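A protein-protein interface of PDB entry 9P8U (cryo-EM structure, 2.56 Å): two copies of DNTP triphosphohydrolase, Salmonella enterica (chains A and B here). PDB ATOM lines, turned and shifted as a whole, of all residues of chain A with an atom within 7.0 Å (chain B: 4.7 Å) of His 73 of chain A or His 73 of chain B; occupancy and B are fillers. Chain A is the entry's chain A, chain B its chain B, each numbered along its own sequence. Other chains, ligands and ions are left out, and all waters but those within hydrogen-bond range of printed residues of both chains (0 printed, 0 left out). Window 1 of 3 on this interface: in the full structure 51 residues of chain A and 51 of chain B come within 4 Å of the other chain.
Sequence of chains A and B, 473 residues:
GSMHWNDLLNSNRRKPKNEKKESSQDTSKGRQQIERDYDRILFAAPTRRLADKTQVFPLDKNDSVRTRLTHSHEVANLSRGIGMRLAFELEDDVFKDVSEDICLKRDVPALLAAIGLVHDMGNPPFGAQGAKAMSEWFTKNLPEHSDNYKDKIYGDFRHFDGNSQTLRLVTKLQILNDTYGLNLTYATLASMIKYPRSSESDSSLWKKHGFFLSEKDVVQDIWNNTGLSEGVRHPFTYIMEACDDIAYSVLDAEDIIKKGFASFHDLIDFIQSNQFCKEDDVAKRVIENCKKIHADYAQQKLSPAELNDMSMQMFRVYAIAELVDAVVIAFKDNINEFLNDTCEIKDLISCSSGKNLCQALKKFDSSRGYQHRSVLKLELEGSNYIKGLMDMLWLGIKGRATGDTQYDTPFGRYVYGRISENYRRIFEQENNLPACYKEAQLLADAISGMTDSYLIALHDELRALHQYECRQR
His 73 of chain A touches one residue of chain B.
Of chain A, only His 73 (3.4 Å) comes within 4 Å of His 73 of chain B.
Of the printed residues of chain A, Asn 77 of chain B touches Tyr 38, Leu 42 and Phe 43.
Of the printed residues of chain B, Tyr 38 of chain A touches Asn 77 (3.5 Å).
Leu 117 of chain B touches none of the printed residues of chain A.
The nearest residue of chain B that does not touch His 73 of chain A is Leu 42 of chain B (4.2 Å).
The nearest printed residue of chain B that does not touch Leu 42 of chain A is His 73 of chain B (4.2 Å).
Among the printed residues, merely in contact across the chains: Tyr 38 of chain A with Asn 77 of chain B, Leu 42 of chain A with Asn 77 of chain B, Phe 43 of chain A with Glu 74 of chain B, Phe 43 of chain A with Asn 77 of chain B, His 73 of chain A with His 73 of chain B and Asn 77 of chain A with Leu 42 of chain B.
Of the 11 printed residues of chain B, 4 touch a printed residue of chain A.
Printed residues of chain A that touch a printed residue of chain B: Tyr 38, Leu 42, Phe 43, His 73 and Asn 77.
Hydrophobic or aromatic side chains of chain A that line the printed part of chain B: Tyr 38, Leu 42, Phe 43 and His 73.
Along chain A the printed residues that touch a printed residue of chain B span positions 38 to 77.
Among the printed residues, 6 pairs touch across the chains.
Among the printed residues, no Asp or Glu carboxylate lies within 4 Å of a Lys or Arg side-chain nitrogen of the other chain.
Leu 42 of chain A touches Asn 77 of chain B, and with the chains exchanged Asn 77 of chain A touches Leu 42 of chain B.
His 73 of chain B touches its own counterpart, His 73 of chain A.
Positions printed for both chains: 42, 69, 70, 71, 72, 73, 74, 75, 76, 77 and 117.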
ATOM      1  N   TYR A  38      32.587   0.522 -15.624  1.00  0.00           N
ATOM      2  CA  TYR A  38      31.750   1.197 -16.610  1.00  0.00           C
ATOM      3  C   TYR A  38      30.276   1.074 -16.246  1.00  0.00           C
ATOM      4  O   TYR A  38      29.510   2.037 -16.364  1.00  0.00           O
ATOM      5  CB  TYR A  38      32.002   0.631 -18.006  1.00  0.00           C
ATOM      6  CG  TYR A  38      31.117   1.247 -19.063  1.00  0.00           C
ATOM      7  CD1 TYR A  38      31.398   2.499 -19.589  1.00  0.00           C
ATOM      8  CD2 TYR A  38      29.994   0.580 -19.531  1.00  0.00           C
ATOM      9  CE1 TYR A  38      30.589   3.066 -20.552  1.00  0.00           C
ATOM     10  CE2 TYR A  38      29.180   1.140 -20.493  1.00  0.00           C
ATOM     11  CZ  TYR A  38      29.483   2.383 -21.000  1.00  0.00           C
ATOM     12  OH  TYR A  38      28.674   2.945 -21.959  1.00  0.00           O
ATOM     13  N   LEU A  42      27.688   4.092 -15.413  1.00  0.00           N
ATOM     14  CA  LEU A  42      26.485   4.273 -16.219  1.00  0.00           C
ATOM     15  C   LEU A  42      25.229   4.300 -15.360  1.00  0.00           C
ATOM     16  O   LEU A  42      24.322   5.105 -15.599  1.00  0.00           O
ATOM     17  CB  LEU A  42      26.386   3.166 -17.266  1.00  0.00           C
ATOM     18  CG  LEU A  42      25.165   3.252 -18.182  1.00  0.00           C
ATOM     19  CD1 LEU A  42      25.309   4.406 -19.157  1.00  0.00           C
ATOM     20  CD2 LEU A  42      24.961   1.947 -18.918  1.00  0.00           C
ATOM     21  N   PHE A  43      25.152   3.431 -14.358  1.00  0.00           N
ATOM     22  CA  PHE A  43      23.957   3.304 -13.538  1.00  0.00           C
ATOM     23  C   PHE A  43      23.913   4.290 -12.379  1.00  0.00           C
ATOM     24  O   PHE A  43      22.937   4.287 -11.623  1.00  0.00           O
ATOM     25  CB  PHE A  43      23.837   1.876 -13.001  1.00  0.00           C
ATOM     26  CG  PHE A  43      23.261   0.906 -13.987  1.00  0.00           C
ATOM     27  CD1 PHE A  43      24.060   0.319 -14.951  1.00  0.00           C
ATOM     28  CD2 PHE A  43      21.917   0.581 -13.952  1.00  0.00           C
ATOM     29  CE1 PHE A  43      23.530  -0.574 -15.859  1.00  0.00           C
ATOM     30  CE2 PHE A  43      21.384  -0.310 -14.857  1.00  0.00           C
ATOM     31  CZ  PHE A  43      22.191  -0.888 -15.811  1.00  0.00           C
ATOM     32  N   THR A  47      25.023  10.188 -13.567  1.00  0.00           N
ATOM     33  CA  THR A  47      25.009   9.917 -15.000  1.00  0.00           C
ATOM     34  C   THR A  47      23.653  10.252 -15.607  1.00  0.00           C
ATOM     35  O   THR A  47      23.578  10.857 -16.681  1.00  0.00           O
ATOM     36  CB  THR A  47      25.360   8.455 -15.266  1.00  0.00           C
ATOM     37  OG1 THR A  47      26.587   8.127 -14.605  1.00  0.00           O
ATOM     38  CG2 THR A  47      25.518   8.213 -16.757  1.00  0.00           C
ATOM     39  N   THR A  67      23.584  17.563 -24.957  1.00  0.00           N
ATOM     40  CA  THR A  67      23.660  17.849 -23.535  1.00  0.00           C
ATOM     41  C   THR A  67      24.914  17.193 -22.969  1.00  0.00           C
ATOM     42  O   THR A  67      25.726  16.620 -23.699  1.00  0.00           O
ATOM     43  CB  THR A  67      22.406  17.359 -22.810  1.00  0.00           C
ATOM     44  OG1 THR A  67      22.419  15.929 -22.744  1.00  0.00           O
ATOM     45  CG2 THR A  67      21.160  17.812 -23.545  1.00  0.00           C
ATOM     46  N   ARG A  68      25.075  17.285 -21.648  1.00  0.00           N
ATOM     47  CA  ARG A  68      26.214  16.636 -21.011  1.00  0.00           C
ATOM     48  C   ARG A  68      26.152  15.126 -21.183  1.00  0.00           C
ATOM     49  O   ARG A  68      27.177  14.477 -21.409  1.00  0.00           O
ATOM     50  CB  ARG A  68      26.276  17.006 -19.530  1.00  0.00           C
ATOM     51  CG  ARG A  68      26.512  18.479 -19.272  1.00  0.00           C
ATOM     52  CD  ARG A  68      27.995  18.795 -19.206  1.00  0.00           C
ATOM     53  NE  ARG A  68      28.249  20.119 -18.652  1.00  0.00           N
ATOM     54  CZ  ARG A  68      28.127  20.435 -17.371  1.00  0.00           C
ATOM     55  NH1 ARG A  68      27.774  19.534 -16.468  1.00  0.00           N
ATOM     56  NH2 ARG A  68      28.369  21.683 -16.984  1.00  0.00           N
ATOM     57  N   LEU A  69      24.953  14.549 -21.082  1.00  0.00           N
ATOM     58  CA  LEU A  69      24.812  13.104 -21.229  1.00  0.00           C
ATOM     59  C   LEU A  69      25.162  12.653 -22.642  1.00  0.00           C
ATOM     60  O   LEU A  69      25.909  11.687 -22.830  1.00  0.00           O
ATOM     61  CB  LEU A  69      23.392  12.677 -20.868  1.00  0.00           C
ATOM     62  CG  LEU A  69      23.126  11.174 -20.924  1.00  0.00           C
ATOM     63  CD1 LEU A  69      24.029  10.439 -19.952  1.00  0.00           C
ATOM     64  CD2 LEU A  69      21.667  10.879 -20.633  1.00  0.00           C
ATOM     65  N   THR A  70      24.625  13.340 -23.653  1.00  0.00           N
ATOM     66  CA  THR A  70      24.893  12.957 -25.035  1.00  0.00           C
ATOM     67  C   THR A  70      26.362  13.149 -25.384  1.00  0.00           C
ATOM     68  O   THR A  70      26.973  12.303 -26.049  1.00  0.00           O
ATOM     69  CB  THR A  70      24.005  13.762 -25.983  1.00  0.00           C
ATOM     70  OG1 THR A  70      22.690  13.870 -25.429  1.00  0.00           O
ATOM     71  CG2 THR A  70      23.924  13.078 -27.332  1.00  0.00           C
ATOM     72  N   HIS A  71      26.948  14.264 -24.946  1.00  0.00           N
ATOM     73  CA  HIS A  71      28.365  14.503 -25.196  1.00  0.00           C
ATOM     74  C   HIS A  71      29.225  13.449 -24.514  1.00  0.00           C
ATOM     75  O   HIS A  71      30.194  12.953 -25.099  1.00  0.00           O
ATOM     76  CB  HIS A  71      28.744  15.905 -24.723  1.00  0.00           C
ATOM     77  CG  HIS A  71      30.211  16.099 -24.511  1.00  0.00           C
ATOM     78  ND1 HIS A  71      31.088  16.329 -25.548  1.00  0.00           N
ATOM     79  CD2 HIS A  71      30.955  16.113 -23.380  1.00  0.00           C
ATOM     80  CE1 HIS A  71      32.309  16.470 -25.066  1.00  0.00           C
ATOM     81  NE2 HIS A  71      32.256  16.343 -23.753  1.00  0.00           N
ATOM     82  N   SER A  72      28.880  13.090 -23.276  1.00  0.00           N
ATOM     83  CA  SER A  72      29.628  12.059 -22.568  1.00  0.00           C
ATOM     84  C   SER A  72      29.520  10.718 -23.276  1.00  0.00           C
ATOM     85  O   SER A  72      30.511   9.990 -23.390  1.00  0.00           O
ATOM     86  CB  SER A  72      29.131  11.947 -21.129  1.00  0.00           C
ATOM     87  OG  SER A  72      29.316  13.166 -20.434  1.00  0.00           O
ATOM     88  N   HIS A  73      28.327  10.372 -23.761  1.00  0.00           N
ATOM     89  CA  HIS A  73      28.165   9.109 -24.473  1.00  0.00           C
ATOM     90  C   HIS A  73      28.955   9.099 -25.775  1.00  0.00           C
ATOM     91  O   HIS A  73      29.545   8.077 -26.140  1.00  0.00           O
ATOM     92  CB  HIS A  73      26.687   8.837 -24.736  1.00  0.00           C
ATOM     93  CG  HIS A  73      26.007   8.095 -23.630  1.00  0.00           C
ATOM     94  ND1 HIS A  73      26.080   6.725 -23.499  1.00  0.00           N
ATOM     95  CD2 HIS A  73      25.245   8.530 -22.599  1.00  0.00           C
ATOM     96  CE1 HIS A  73      25.391   6.348 -22.437  1.00  0.00           C
ATOM     97  NE2 HIS A  73      24.874   7.424 -21.873  1.00  0.00           N
ATOM     98  N   GLU A  74      28.974  10.223 -26.493  1.00  0.00           N
ATOM     99  CA  GLU A  74      29.748  10.296 -27.729  1.00  0.00           C
ATOM    100  C   GLU A  74      31.244  10.175 -27.458  1.00  0.00           C
ATOM    101  O   GLU A  74      31.961   9.477 -28.189  1.00  0.00           O
ATOM    102  CB  GLU A  74      29.424  11.595 -28.460  1.00  0.00           C
ATOM    103  CG  GLU A  74      28.328  11.447 -29.502  1.00  0.00           C
ATOM    104  CD  GLU A  74      27.211  12.459 -29.330  1.00  0.00           C
ATOM    105  OE1 GLU A  74      27.467  13.547 -28.774  1.00  0.00           O
ATOM    106  OE2 GLU A  74      26.075  12.164 -29.756  1.00  0.00           O
ATOM    107  N   VAL A  75      31.732  10.840 -26.409  1.00  0.00           N
ATOM    108  CA  VAL A  75      33.139  10.712 -26.038  1.00  0.00           C
ATOM    109  C   VAL A  75      33.452   9.274 -25.649  1.00  0.00           C
ATOM    110  O   VAL A  75      34.498   8.728 -26.018  1.00  0.00           O
ATOM    111  CB  VAL A  75      33.487  11.693 -24.905  1.00  0.00           C
ATOM    112  CG1 VAL A  75      34.890  11.435 -24.393  1.00  0.00           C
ATOM    113  CG2 VAL A  75      33.361  13.120 -25.391  1.00  0.00           C
ATOM    114  N   ALA A  76      32.548   8.640 -24.899  1.00  0.00           N
ATOM    115  CA  ALA A  76      32.753   7.254 -24.501  1.00  0.00           C
ATOM    116  C   ALA A  76      32.802   6.335 -25.711  1.00  0.00           C
ATOM    117  O   ALA A  76      33.620   5.415 -25.763  1.00  0.00           O
ATOM    118  CB  ALA A  76      31.651   6.817 -23.539  1.00  0.00           C
ATOM    119  N   ASN A  77      31.932   6.566 -26.692  1.00  0.00           N
ATOM    120  CA  ASN A  77      31.945   5.755 -27.903  1.00  0.00           C
ATOM    121  C   ASN A  77      33.226   5.934 -28.705  1.00  0.00           C
ATOM    122  O   ASN A  77      33.786   4.947 -29.196  1.00  0.00           O
ATOM    123  CB  ASN A  77      30.739   6.090 -28.775  1.00  0.00           C
ATOM    124  CG  ASN A  77      30.592   5.146 -29.946  1.00  0.00           C
ATOM    125  OD1 ASN A  77      30.491   3.933 -29.771  1.00  0.00           O
ATOM    126  ND2 ASN A  77      30.583   5.697 -31.152  1.00  0.00           N
ATOM    127  N   LEU A  78      33.700   7.173 -28.856  1.00  0.00           N
ATOM    128  CA  LEU A  78      34.957   7.384 -29.569  1.00  0.00           C
ATOM    129  C   LEU A  78      36.122   6.723 -28.840  1.00  0.00           C
ATOM    130  O   LEU A  78      36.977   6.080 -29.467  1.00  0.00           O
ATOM    131  CB  LEU A  78      35.213   8.878 -29.750  1.00  0.00           C
ATOM    132  CG  LEU A  78      34.219   9.623 -30.638  1.00  0.00           C
ATOM    133  CD1 LEU A  78      34.489  11.114 -30.603  1.00  0.00           C
ATOM    134  CD2 LEU A  78      34.282   9.101 -32.060  1.00  0.00           C
ATOM    135  N   SER A  79      36.167   6.863 -27.513  1.00  0.00           N
ATOM    136  CA  SER A  79      37.223   6.223 -26.738  1.00  0.00           C
ATOM    137  C   SER A  79      37.141   4.708 -26.849  1.00  0.00           C
ATOM    138  O   SER A  79      38.168   4.030 -26.943  1.00  0.00           O
ATOM    139  CB  SER A  79      37.139   6.662 -25.278  1.00  0.00           C
ATOM    140  OG  SER A  79      37.189   8.073 -25.171  1.00  0.00           O
ATOM    141  N   ALA A 113      36.031   3.639 -22.519  1.00  0.00           N
ATOM    142  CA  ALA A 113      34.632   4.048 -22.477  1.00  0.00           C
ATOM    143  C   ALA A 113      34.251   4.579 -21.101  1.00  0.00           C
ATOM    144  O   ALA A 113      33.533   5.580 -20.991  1.00  0.00           O
ATOM    145  CB  ALA A 113      33.732   2.878 -22.868  1.00  0.00           C
ATOM    146  N   GLY A 116      35.770   7.993 -20.577  1.00  0.00           N
ATOM    147  CA  GLY A 116      35.098   8.966 -21.420  1.00  0.00           C
ATOM    148  C   GLY A 116      33.725   9.347 -20.900  1.00  0.00           C
ATOM    149  O   GLY A 116      33.329  10.513 -20.964  1.00  0.00           O
ATOM    150  N   LEU A 117      32.982   8.370 -20.377  1.00  0.00           N
ATOM    151  CA  LEU A 117      31.624   8.638 -19.916  1.00  0.00           C
ATOM    152  C   LEU A 117      31.610   9.487 -18.650  1.00  0.00           C
ATOM    153  O   LEU A 117      30.674  10.266 -18.440  1.00  0.00           O
ATOM    154  CB  LEU A 117      30.887   7.319 -19.680  1.00  0.00           C
ATOM    155  CG  LEU A 117      29.449   7.395 -19.171  1.00  0.00           C
ATOM    156  CD1 LEU A 117      28.551   8.043 -20.204  1.00  0.00           C
ATOM    157  CD2 LEU A 117      28.941   6.010 -18.816  1.00  0.00           C
ATOM    158  N   HIS A 119      34.014  11.685 -17.728  1.00  0.00           N
ATOM    159  CA  HIS A 119      34.974  12.779 -17.810  1.00  0.00           C
ATOM    160  C   HIS A 119      34.389  14.123 -17.392  1.00  0.00           C
ATOM    161  O   HIS A 119      35.142  14.998 -16.954  1.00  0.00           O
ATOM    162  CB  HIS A 119      35.538  12.878 -19.228  1.00  0.00           C
ATOM    163  CG  HIS A 119      34.728  13.738 -20.146  1.00  0.00           C
ATOM    164  ND1 HIS A 119      33.599  13.284 -20.790  1.00  0.00           N
ATOM    165  CD2 HIS A 119      34.891  15.024 -20.534  1.00  0.00           C
ATOM    166  CE1 HIS A 119      33.097  14.253 -21.533  1.00  0.00           C
ATOM    167  NE2 HIS A 119      33.862  15.321 -21.395  1.00  0.00           N
ATOM    168  N   LEU B  42      23.798   5.455 -32.704  1.00  0.00           N
ATOM    169  CA  LEU B  42      24.089   6.384 -31.617  1.00  0.00           C
ATOM    170  C   LEU B  42      24.095   7.830 -32.097  1.00  0.00           C
ATOM    171  O   LEU B  42      23.577   8.718 -31.412  1.00  0.00           O
ATOM    172  CB  LEU B  42      25.427   6.032 -30.972  1.00  0.00           C
ATOM    173  CG  LEU B  42      25.841   6.921 -29.802  1.00  0.00           C
ATOM    174  CD1 LEU B  42      24.899   6.730 -28.630  1.00  0.00           C
ATOM    175  CD2 LEU B  42      27.267   6.628 -29.394  1.00  0.00           C
ATOM    176  N   LEU B  69      15.864   7.581 -23.585  1.00  0.00           N
ATOM    177  CA  LEU B  69      17.286   7.491 -23.901  1.00  0.00           C
ATOM    178  C   LEU B  69      18.037   6.690 -22.844  1.00  0.00           C
ATOM    179  O   LEU B  69      18.840   5.809 -23.170  1.00  0.00           O
ATOM    180  CB  LEU B  69      17.879   8.891 -24.036  1.00  0.00           C
ATOM    181  CG  LEU B  69      19.353   8.951 -24.433  1.00  0.00           C
ATOM    182  CD1 LEU B  69      19.582   8.196 -25.729  1.00  0.00           C
ATOM    183  CD2 LEU B  69      19.813  10.391 -24.559  1.00  0.00           C
ATOM    184  N   THR B  70      17.789   6.988 -21.567  1.00  0.00           N
ATOM    185  CA  THR B  70      18.470   6.269 -20.495  1.00  0.00           C
ATOM    186  C   THR B  70      18.083   4.797 -20.489  1.00  0.00           C
ATOM    187  O   THR B  70      18.937   3.921 -20.303  1.00  0.00           O
ATOM    188  CB  THR B  70      18.152   6.913 -19.148  1.00  0.00           C
ATOM    189  OG1 THR B  70      18.553   8.289 -19.169  1.00  0.00           O
ATOM    190  CG2 THR B  70      18.889   6.200 -18.031  1.00  0.00           C
ATOM    191  N   HIS B  71      16.797   4.507 -20.690  1.00  0.00           N
ATOM    192  CA  HIS B  71      16.346   3.120 -20.741  1.00  0.00           C
ATOM    193  C   HIS B  71      16.988   2.376 -21.903  1.00  0.00           C
ATOM    194  O   HIS B  71      17.429   1.231 -21.751  1.00  0.00           O
ATOM    195  CB  HIS B  71      14.822   3.079 -20.844  1.00  0.00           C
ATOM    196  CG  HIS B  71      14.280   1.766 -21.310  1.00  0.00           C
ATOM    197  ND1 HIS B  71      14.133   0.683 -20.472  1.00  0.00           N
ATOM    198  CD2 HIS B  71      13.836   1.364 -22.524  1.00  0.00           C
ATOM    199  CE1 HIS B  71      13.628  -0.331 -21.150  1.00  0.00           C
ATOM    200  NE2 HIS B  71      13.439   0.055 -22.398  1.00  0.00           N
ATOM    201  N   SER B  72      17.057   3.016 -23.072  1.00  0.00           N
ATOM    202  CA  SER B  72      17.693   2.389 -24.223  1.00  0.00           C
ATOM    203  C   SER B  72      19.169   2.134 -23.962  1.00  0.00           C
ATOM    204  O   SER B  72      19.698   1.081 -24.331  1.00  0.00           O
ATOM    205  CB  SER B  72      17.511   3.262 -25.462  1.00  0.00           C
ATOM    206  OG  SER B  72      16.141   3.524 -25.702  1.00  0.00           O
ATOM    207  N   HIS B  73      19.852   3.085 -23.323  1.00  0.00           N
ATOM    208  CA  HIS B  73      21.270   2.897 -23.030  1.00  0.00           C
ATOM    209  C   HIS B  73      21.487   1.762 -22.039  1.00  0.00           C
ATOM    210  O   HIS B  73      22.433   0.981 -22.181  1.00  0.00           O
ATOM    211  CB  HIS B  73      21.873   4.197 -22.509  1.00  0.00           C
ATOM    212  CG  HIS B  73      22.349   5.111 -23.594  1.00  0.00           C
ATOM    213  ND1 HIS B  73      23.259   4.718 -24.549  1.00  0.00           N
ATOM    214  CD2 HIS B  73      22.033   6.395 -23.880  1.00  0.00           C
ATOM    215  CE1 HIS B  73      23.488   5.722 -25.375  1.00  0.00           C
ATOM    216  NE2 HIS B  73      22.756   6.753 -24.991  1.00  0.00           N
ATOM    217  N   GLU B  74      20.625   1.653 -21.028  1.00  0.00           N
ATOM    218  CA  GLU B  74      20.748   0.557 -20.072  1.00  0.00           C
ATOM    219  C   GLU B  74      20.493  -0.789 -20.743  1.00  0.00           C
ATOM    220  O   GLU B  74      21.197  -1.773 -20.478  1.00  0.00           O
ATOM    221  CB  GLU B  74      19.790   0.773 -18.904  1.00  0.00           C
ATOM    222  CG  GLU B  74      20.397   1.568 -17.763  1.00  0.00           C
ATOM    223  CD  GLU B  74      19.443   2.598 -17.198  1.00  0.00           C
ATOM    224  OE1 GLU B  74      18.363   2.795 -17.792  1.00  0.00           O
ATOM    225  OE2 GLU B  74      19.771   3.213 -16.162  1.00  0.00           O
ATOM    226  N   VAL B  75      19.488  -0.851 -21.620  1.00  0.00           N
ATOM    227  CA  VAL B  75      19.215  -2.084 -22.357  1.00  0.00           C
ATOM    228  C   VAL B  75      20.410  -2.450 -23.227  1.00  0.00           C
ATOM    229  O   VAL B  75      20.811  -3.619 -23.313  1.00  0.00           O
ATOM    230  CB  VAL B  75      17.932  -1.939 -23.194  1.00  0.00           C
ATOM    231  CG1 VAL B  75      17.788  -3.104 -24.155  1.00  0.00           C
ATOM    232  CG2 VAL B  75      16.720  -1.848 -22.291  1.00  0.00           C
ATOM    233  N   ALA B  76      20.995  -1.449 -23.887  1.00  0.00           N
ATOM    234  CA  ALA B  76      22.160  -1.690 -24.730  1.00  0.00           C
ATOM    235  C   ALA B  76      23.335  -2.201 -23.908  1.00  0.00           C
ATOM    236  O   ALA B  76      24.067  -3.093 -24.343  1.00  0.00           O
ATOM    237  CB  ALA B  76      22.540  -0.411 -25.474  1.00  0.00           C
ATOM    238  N   ASN B  77      23.535  -1.638 -22.715  1.00  0.00           N
ATOM    239  CA  ASN B  77      24.626  -2.091 -21.858  1.00  0.00           C
ATOM    240  C   ASN B  77      24.418  -3.534 -21.415  1.00  0.00           C
ATOM    241  O   ASN B  77      25.359  -4.337 -21.410  1.00  0.00           O
ATOM    242  CB  ASN B  77      24.755  -1.174 -20.645  1.00  0.00           C
ATOM    243  CG  ASN B  77      25.954  -1.515 -19.791  1.00  0.00           C
ATOM    244  OD1 ASN B  77      27.075  -1.614 -20.287  1.00  0.00           O
ATOM    245  ND2 ASN B  77      25.725  -1.699 -18.498  1.00  0.00           N
ATOM    246  N   LEU B 117      19.986  -0.562 -28.208  1.00  0.00           N
ATOM    247  CA  LEU B 117      19.887   0.893 -28.200  1.00  0.00           C
ATOM    248  C   LEU B 117      18.742   1.395 -29.069  1.00  0.00           C
ATOM    249  O   LEU B 117      18.098   2.391 -28.726  1.00  0.00           O
ATOM    250  CB  LEU B 117      21.209   1.505 -28.662  1.00  0.00           C
ATOM    251  CG  LEU B 117      21.294   3.030 -28.678  1.00  0.00           C
ATOM    252  CD1 LEU B 117      21.050   3.593 -27.292  1.00  0.00           C
ATOM    253  CD2 LEU B 117      22.643   3.477 -29.208  1.00  0.00           C
